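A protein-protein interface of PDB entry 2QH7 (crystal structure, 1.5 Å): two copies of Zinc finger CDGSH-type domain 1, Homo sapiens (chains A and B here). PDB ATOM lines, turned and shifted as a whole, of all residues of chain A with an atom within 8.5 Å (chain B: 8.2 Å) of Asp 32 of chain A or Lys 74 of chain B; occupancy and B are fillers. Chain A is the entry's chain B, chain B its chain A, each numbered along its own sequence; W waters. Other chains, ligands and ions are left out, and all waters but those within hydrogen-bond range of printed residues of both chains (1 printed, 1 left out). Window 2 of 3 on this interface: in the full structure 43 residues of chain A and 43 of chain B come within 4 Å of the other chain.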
ATOM      1  N   ALA A  27     -14.875  -8.228   7.645  1.00  0.00           N
ATOM      2  CA  ALA A  27     -13.496  -8.596   7.862  1.00  0.00           C
ATOM      3  C   ALA A  27     -13.372  -9.795   8.754  1.00  0.00           C
ATOM      4  O   ALA A  27     -13.835  -9.795   9.897  1.00  0.00           O
ATOM      5  CB  ALA A  27     -12.691  -7.423   8.395  1.00  0.00           C
ATOM      6  N   PHE A  28     -12.727 -10.822   8.217  1.00  0.00           N
ATOM      7  CA  PHE A  28     -12.549 -12.099   8.900  1.00  0.00           C
ATOM      8  C   PHE A  28     -11.093 -12.474   9.046  1.00  0.00           C
ATOM      9  O   PHE A  28     -10.294 -12.274   8.130  1.00  0.00           O
ATOM     10  CB  PHE A  28     -13.241 -13.210   8.105  1.00  0.00           C
ATOM     11  CG  PHE A  28     -14.721 -13.050   7.996  1.00  0.00           C
ATOM     12  CD1 PHE A  28     -15.527 -13.375   9.077  1.00  0.00           C
ATOM     13  CD2 PHE A  28     -15.320 -12.605   6.816  1.00  0.00           C
ATOM     14  CE1 PHE A  28     -16.908 -13.243   8.982  1.00  0.00           C
ATOM     15  CE2 PHE A  28     -16.702 -12.469   6.710  1.00  0.00           C
ATOM     16  CZ  PHE A  28     -17.490 -12.784   7.813  1.00  0.00           C
ATOM     17  N   ASP A  29     -10.771 -13.049  10.202  1.00  0.00           N
ATOM     18  CA  ASP A  29      -9.453 -13.617  10.502  1.00  0.00           C
ATOM     19  C   ASP A  29      -9.383 -15.034   9.947  1.00  0.00           C
ATOM     20  O   ASP A  29     -10.290 -15.825  10.181  1.00  0.00           O
ATOM     21  CB  ASP A  29      -9.196 -13.648  12.000  1.00  0.00           C
ATOM     22  CG  ASP A  29      -9.100 -12.264  12.603  1.00  0.00           C
ATOM     23  OD1 ASP A  29      -8.846 -11.304  11.849  1.00  0.00           O
ATOM     24  OD2 ASP A  29      -9.279 -12.134  13.830  1.00  0.00           O
ATOM     25  N   MET A  30      -8.313 -15.352   9.210  1.00  0.00           N
ATOM     26  CA  MET A  30      -8.246 -16.626   8.473  1.00  0.00           C
ATOM     27  C   MET A  30      -8.111 -17.816   9.409  1.00  0.00           C
ATOM     28  O   MET A  30      -8.521 -18.915   9.061  1.00  0.00           O
ATOM     29  CB  MET A  30      -7.157 -16.620   7.382  1.00  0.00           C
ATOM     30  CG  MET A  30      -5.760 -16.222   7.810  1.00  0.00           C
ATOM     31  SD  MET A  30      -4.612 -15.992   6.422  1.00  0.00           S
ATOM     32  CE  MET A  30      -5.184 -14.462   5.701  1.00  0.00           C
ATOM     33  N   GLU A  31      -7.604 -17.572  10.614  1.00  0.00           N
ATOM     34  CA  GLU A  31      -7.535 -18.591  11.656  1.00  0.00           C
ATOM     35  C   GLU A  31      -8.919 -18.958  12.213  1.00  0.00           C
ATOM     36  O   GLU A  31      -9.079 -20.033  12.787  1.00  0.00           O
ATOM     37  CB  GLU A  31      -6.634 -18.128  12.806  1.00  0.00           C
ATOM     38  CG  GLU A  31      -5.175 -17.850  12.405  1.00  0.00           C
ATOM     39  CD  GLU A  31      -4.924 -16.412  11.956  1.00  0.00           C
ATOM     40  OE1 GLU A  31      -5.913 -15.688  11.686  1.00  0.00           O
ATOM     41  OE2 GLU A  31      -3.736 -16.000  11.877  1.00  0.00           O
ATOM     42  N   ASP A  32      -9.897 -18.063  12.069  1.00  0.00           N
ATOM     43  CA  ASP A  32     -11.278 -18.340  12.455  1.00  0.00           C
ATOM     44  C   ASP A  32     -12.061 -19.055  11.351  1.00  0.00           C
ATOM     45  O   ASP A  32     -13.213 -19.418  11.568  1.00  0.00           O
ATOM     46  CB  ASP A  32     -12.017 -17.042  12.810  1.00  0.00           C
ATOM     47  CG  ASP A  32     -11.436 -16.328  14.030  1.00  0.00           C
ATOM     48  OD1 ASP A  32     -10.664 -16.942  14.814  1.00  0.00           O
ATOM     49  OD2 ASP A  32     -11.786 -15.136  14.223  1.00  0.00           O
ATOM     50  N   LEU A  33     -11.462 -19.241  10.172  1.00  0.00           N
ATOM     51  CA  LEU A  33     -12.157 -19.889   9.054  1.00  0.00           C
ATOM     52  C   LEU A  33     -11.965 -21.387   9.149  1.00  0.00           C
ATOM     53  O   LEU A  33     -10.975 -21.859   9.699  1.00  0.00           O
ATOM     54  CB  LEU A  33     -11.650 -19.387   7.691  1.00  0.00           C
ATOM     55  CG  LEU A  33     -11.759 -17.894   7.356  1.00  0.00           C
ATOM     56  CD1 LEU A  33     -11.419 -17.630   5.890  1.00  0.00           C
ATOM     57  CD2 LEU A  33     -13.131 -17.348   7.675  1.00  0.00           C
ATOM     58  N   GLY A  34     -12.912 -22.140   8.609  1.00  0.00           N
ATOM     59  CA  GLY A  34     -12.799 -23.588   8.600  1.00  0.00           C
ATOM     60  C   GLY A  34     -11.885 -24.058   7.483  1.00  0.00           C
ATOM     61  O   GLY A  34     -10.867 -23.425   7.182  1.00  0.00           O
ATOM     62  N   ASP A  35     -12.254 -25.179   6.871  1.00  0.00           N
ATOM     63  CA  ASP A  35     -11.610 -25.627   5.648  1.00  0.00           C
ATOM     64  C   ASP A  35     -11.942 -24.704   4.466  1.00  0.00           C
ATOM     65  O   ASP A  35     -11.087 -24.446   3.627  1.00  0.00           O
ATOM     66  CB  ASP A  35     -12.041 -27.061   5.328  1.00  0.00           C
ATOM     67  N   LYS A  36     -13.179 -24.211   4.410  1.00  0.00           N
ATOM     68  CA  LYS A  36     -13.673 -23.509   3.238  1.00  0.00           C
ATOM     69  C   LYS A  36     -14.756 -22.489   3.603  1.00  0.00           C
ATOM     70  O   LYS A  36     -15.668 -22.789   4.381  1.00  0.00           O
ATOM     71  CB  LYS A  36     -14.235 -24.525   2.242  1.00  0.00           C
ATOM     72  CG  LYS A  36     -14.753 -23.935   0.942  1.00  0.00           C
ATOM     73  CD  LYS A  36     -14.932 -25.031  -0.106  1.00  0.00           C
ATOM     74  CE  LYS A  36     -15.686 -24.541  -1.332  1.00  0.00           C
ATOM     75  NZ  LYS A  36     -15.426 -25.416  -2.523  1.00  0.00           N
ATOM     76  N   ALA A  37     -14.637 -21.285   3.044  1.00  0.00           N
ATOM     77  CA  ALA A  37     -15.670 -20.271   3.129  1.00  0.00           C
ATOM     78  C   ALA A  37     -15.942 -19.719   1.731  1.00  0.00           C
ATOM     79  O   ALA A  37     -15.026 -19.465   0.952  1.00  0.00           O
ATOM     80  CB  ALA A  37     -15.242 -19.158   4.064  1.00  0.00           C
ATOM     81  N   TYR A  39     -17.913 -16.728  -0.177  1.00  0.00           N
ATOM     82  CA  TYR A  39     -18.462 -15.388   0.044  1.00  0.00           C
ATOM     83  C   TYR A  39     -19.249 -14.873  -1.157  1.00  0.00           C
ATOM     84  O   TYR A  39     -18.790 -14.973  -2.316  1.00  0.00           O
ATOM     85  CB  TYR A  39     -17.344 -14.431   0.458  1.00  0.00           C
ATOM     86  CG  TYR A  39     -16.622 -14.845   1.719  1.00  0.00           C
ATOM     87  CD1 TYR A  39     -17.190 -14.648   2.988  1.00  0.00           C
ATOM     88  CD2 TYR A  39     -15.372 -15.433   1.651  1.00  0.00           C
ATOM     89  CE1 TYR A  39     -16.507 -15.016   4.127  1.00  0.00           C
ATOM     90  CE2 TYR A  39     -14.688 -15.793   2.776  1.00  0.00           C
ATOM     91  CZ  TYR A  39     -15.266 -15.589   4.018  1.00  0.00           C
ATOM     92  OH  TYR A  39     -14.590 -15.990   5.140  1.00  0.00           O
ATOM     93  N   MET B  30      -5.622 -20.045   1.666  1.00  0.00           N
ATOM     94  CA  MET B  30      -5.206 -19.159   2.770  1.00  0.00           C
ATOM     95  C   MET B  30      -3.693 -19.021   2.915  1.00  0.00           C
ATOM     96  O   MET B  30      -3.192 -17.993   3.353  1.00  0.00           O
ATOM     97  CB  MET B  30      -5.730 -19.696   4.108  1.00  0.00           C
ATOM     98  CG  MET B  30      -7.209 -19.496   4.348  1.00  0.00           C
ATOM     99  SD  MET B  30      -7.707 -20.403   5.828  1.00  0.00           S
ATOM    100  CE  MET B  30      -9.390 -20.826   5.371  1.00  0.00           C
ATOM    101  N   ASP B  35      -0.694 -11.130   4.956  1.00  0.00           N
ATOM    102  CA  ASP B  35      -1.378 -10.697   6.181  1.00  0.00           C
ATOM    103  C   ASP B  35      -2.793 -10.203   5.982  1.00  0.00           C
ATOM    104  O   ASP B  35      -3.623 -10.359   6.865  1.00  0.00           O
ATOM    105  CB  ASP B  35      -0.592  -9.579   6.847  1.00  0.00           C
ATOM    106  CG  ASP B  35       0.737 -10.040   7.349  1.00  0.00           C
ATOM    107  OD1 ASP B  35       1.048 -11.241   7.180  1.00  0.00           O
ATOM    108  OD2 ASP B  35       1.465  -9.197   7.905  1.00  0.00           O
ATOM    109  N   ILE B  71      -9.915 -10.467   4.277  1.00  0.00           N
ATOM    110  CA  ILE B  71      -9.420 -11.695   4.891  1.00  0.00           C
ATOM    111  C   ILE B  71      -8.053 -11.367   5.446  1.00  0.00           C
ATOM    112  O   ILE B  71      -7.201 -10.894   4.711  1.00  0.00           O
ATOM    113  CB  ILE B  71      -9.324 -12.841   3.851  1.00  0.00           C
ATOM    114  CG1 ILE B  71     -10.681 -13.130   3.222  1.00  0.00           C
ATOM    115  CG2 ILE B  71      -8.747 -14.090   4.511  1.00  0.00           C
ATOM    116  CD1 ILE B  71     -11.767 -13.553   4.191  1.00  0.00           C
ATOM    117  N   LYS B  72      -7.844 -11.611   6.736  1.00  0.00           N
ATOM    118  CA  LYS B  72      -6.643 -11.152   7.403  1.00  0.00           C
ATOM    119  C   LYS B  72      -6.129 -12.118   8.450  1.00  0.00           C
ATOM    120  O   LYS B  72      -6.801 -13.047   8.846  1.00  0.00           O
ATOM    121  CB  LYS B  72      -6.891  -9.767   8.008  1.00  0.00           C
ATOM    122  CG  LYS B  72      -7.926  -9.719   9.125  1.00  0.00           C
ATOM    123  CD  LYS B  72      -8.262  -8.283   9.505  1.00  0.00           C
ATOM    124  CE  LYS B  72      -9.107  -8.203  10.779  1.00  0.00           C
ATOM    125  NZ  LYS B  72      -8.375  -8.575  12.015  1.00  0.00           N
ATOM    126  N   LYS B  73      -4.896 -11.896   8.870  1.00  0.00           N
ATOM    127  CA  LYS B  73      -4.304 -12.620   9.981  1.00  0.00           C
ATOM    128  C   LYS B  73      -4.744 -11.964  11.284  1.00  0.00           C
ATOM    129  O   LYS B  73      -4.805 -10.742  11.375  1.00  0.00           O
ATOM    130  CB  LYS B  73      -2.784 -12.613   9.861  1.00  0.00           C
ATOM    131  CG  LYS B  73      -2.247 -13.462   8.716  1.00  0.00           C
ATOM    132  CD  LYS B  73      -2.152 -14.942   9.098  1.00  0.00           C
ATOM    133  CE  LYS B  73      -0.991 -15.664   8.395  1.00  0.00           C
ATOM    134  NZ  LYS B  73      -1.230 -15.943   6.963  1.00  0.00           N
ATOM    135  N   LYS B  74      -5.097 -12.792  12.261  1.00  0.00           N
ATOM    136  CA  LYS B  74      -5.408 -12.338  13.609  1.00  0.00           C
ATOM    137  C   LYS B  74      -4.141 -11.784  14.252  1.00  0.00           C
ATOM    138  O   LYS B  74      -4.089 -10.605  14.606  1.00  0.00           O
ATOM    139  CB  LYS B  74      -5.964 -13.500  14.453  1.00  0.00           C
ATOM    140  CG  LYS B  74      -6.579 -13.078  15.791  1.00  0.00           C
ATOM    141  CD  LYS B  74      -7.178 -14.259  16.575  1.00  0.00           C
ATOM    142  CE  LYS B  74      -8.455 -14.793  15.938  1.00  0.00           C
HETATM  143  O   HOH W   1      -8.087  -9.911  14.990  1.00  0.00           O
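N of Lys 72 of chain B sits at hydrogen-bond distance from O of Phe 28 of chain A (2.9 Å). The side-chain amino group (NZ) of Lys 72 of chain B is in salt-bridge range of the side-chain carboxylate (OD1) of Asp 29 of chain A (2.8 Å). The backbone NH (N) of Met 30 of chain A sits at hydrogen-bond distance from the backbone carbonyl oxygen (O) of Lys 72 of chain B, at 2.8 Å. NZ of Lys 73 of chain B lies within hydrogen-bond range of SD of Met 30 of chain A, 3.4 Å away. The backbone NH (N) of Lys 74 of chain B is in hydrogen-bond range of the side-chain carboxylate (OE1) of Glu 31 of chain A, 3.1 Å away. The backbone carbonyl oxygen (O) of Met 30 of chain A sits close to the side-chain sulfur (SD) of Met 30 of chain B (3.7 Å).
The backbone NH (N) of Lys 73 of chain B lies within hydrogen-bond range of the backbone carbonyl oxygen (O) of Asp 35 of chain B (2.8 Å).
Phe 28 of chain A touches Ile 71 of chain B (O to CA, 3.4 Å). Lys 74 of chain B touches Asp 29 of chain A. CG2 of Ile 71 of chain B touches CE of Met 30 of chain A, at 3.8 Å. O of Lys 72 of chain B touches OE1 of Glu 31 of chain A, at 3.98 Å. OE2 of Glu 31 of chain A touches CD of Lys 73 of chain B, at 3.4 Å. CE of Lys 74 of chain B touches OD1 of Asp 32 of chain A, at 3.3 Å. CB of Leu 33 of chain A touches CE of Met 30 of chain B, at 3.5 Å. Met 30 of chain B touches Gly 34 of chain A (CE to O, 3.5 Å). CD1 of Ile 71 of chain B touches OH of Tyr 39 of chain A, at 3.8 Å.
Printed residues of chain B within 4 Å of Phe 28 of chain A: Ile 71 and Lys 72. Printed residues of chain B within 4 Å of Met 30 of chain A: Met 30, Ile 71, Lys 72 and Lys 73. Printed residues of chain B within 4 Å of Glu 31 of chain A: Lys 72 (3.98 Å), Lys 73 (3.4 Å) and Lys 74 (3.1 Å). Of chain B, only Lys 74 comes within 4 Å of Asp 32 of chain A. Printed residues of chain B within 4 Å of Leu 33 of chain A: Met 30. Asp 35 of chain B touches none of the printed residues of chain A. Of chain A, only Asp 29, Glu 31 and Asp 32 come within 4 Å of Lys 74 of chain B.
Of the 6 printed residues of chain B, 5 touch a printed residue of chain A. Printed residues of chain B that touch a printed residue of chain A: Met 30, Ile 71, Lys 72, Lys 73 and Lys 74. Hydrophobic or aromatic side chains of chain A that line the printed part of chain B: Met 30, Leu 33 and Tyr 39. Along chain A the printed residues that touch a printed residue of chain B span positions 28 to 39. Among the printed residues, 15 pairs touch across the chains. Among the printed residues, Asp or Glu carboxylates within 4 Å of a Lys or Arg side-chain nitrogen of the other chain: Asp 29 of chain A with Lys 72 of chain B.
Met 30 of chain B touches its own counterpart, Met 30 of chain A.
Water W1 lies within hydrogen-bond range of the side-chain carboxylate of Asp 29 of chain A (2.8 Å) and the side-chain amino group of Lys 72 of chain B (3.3 Å).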
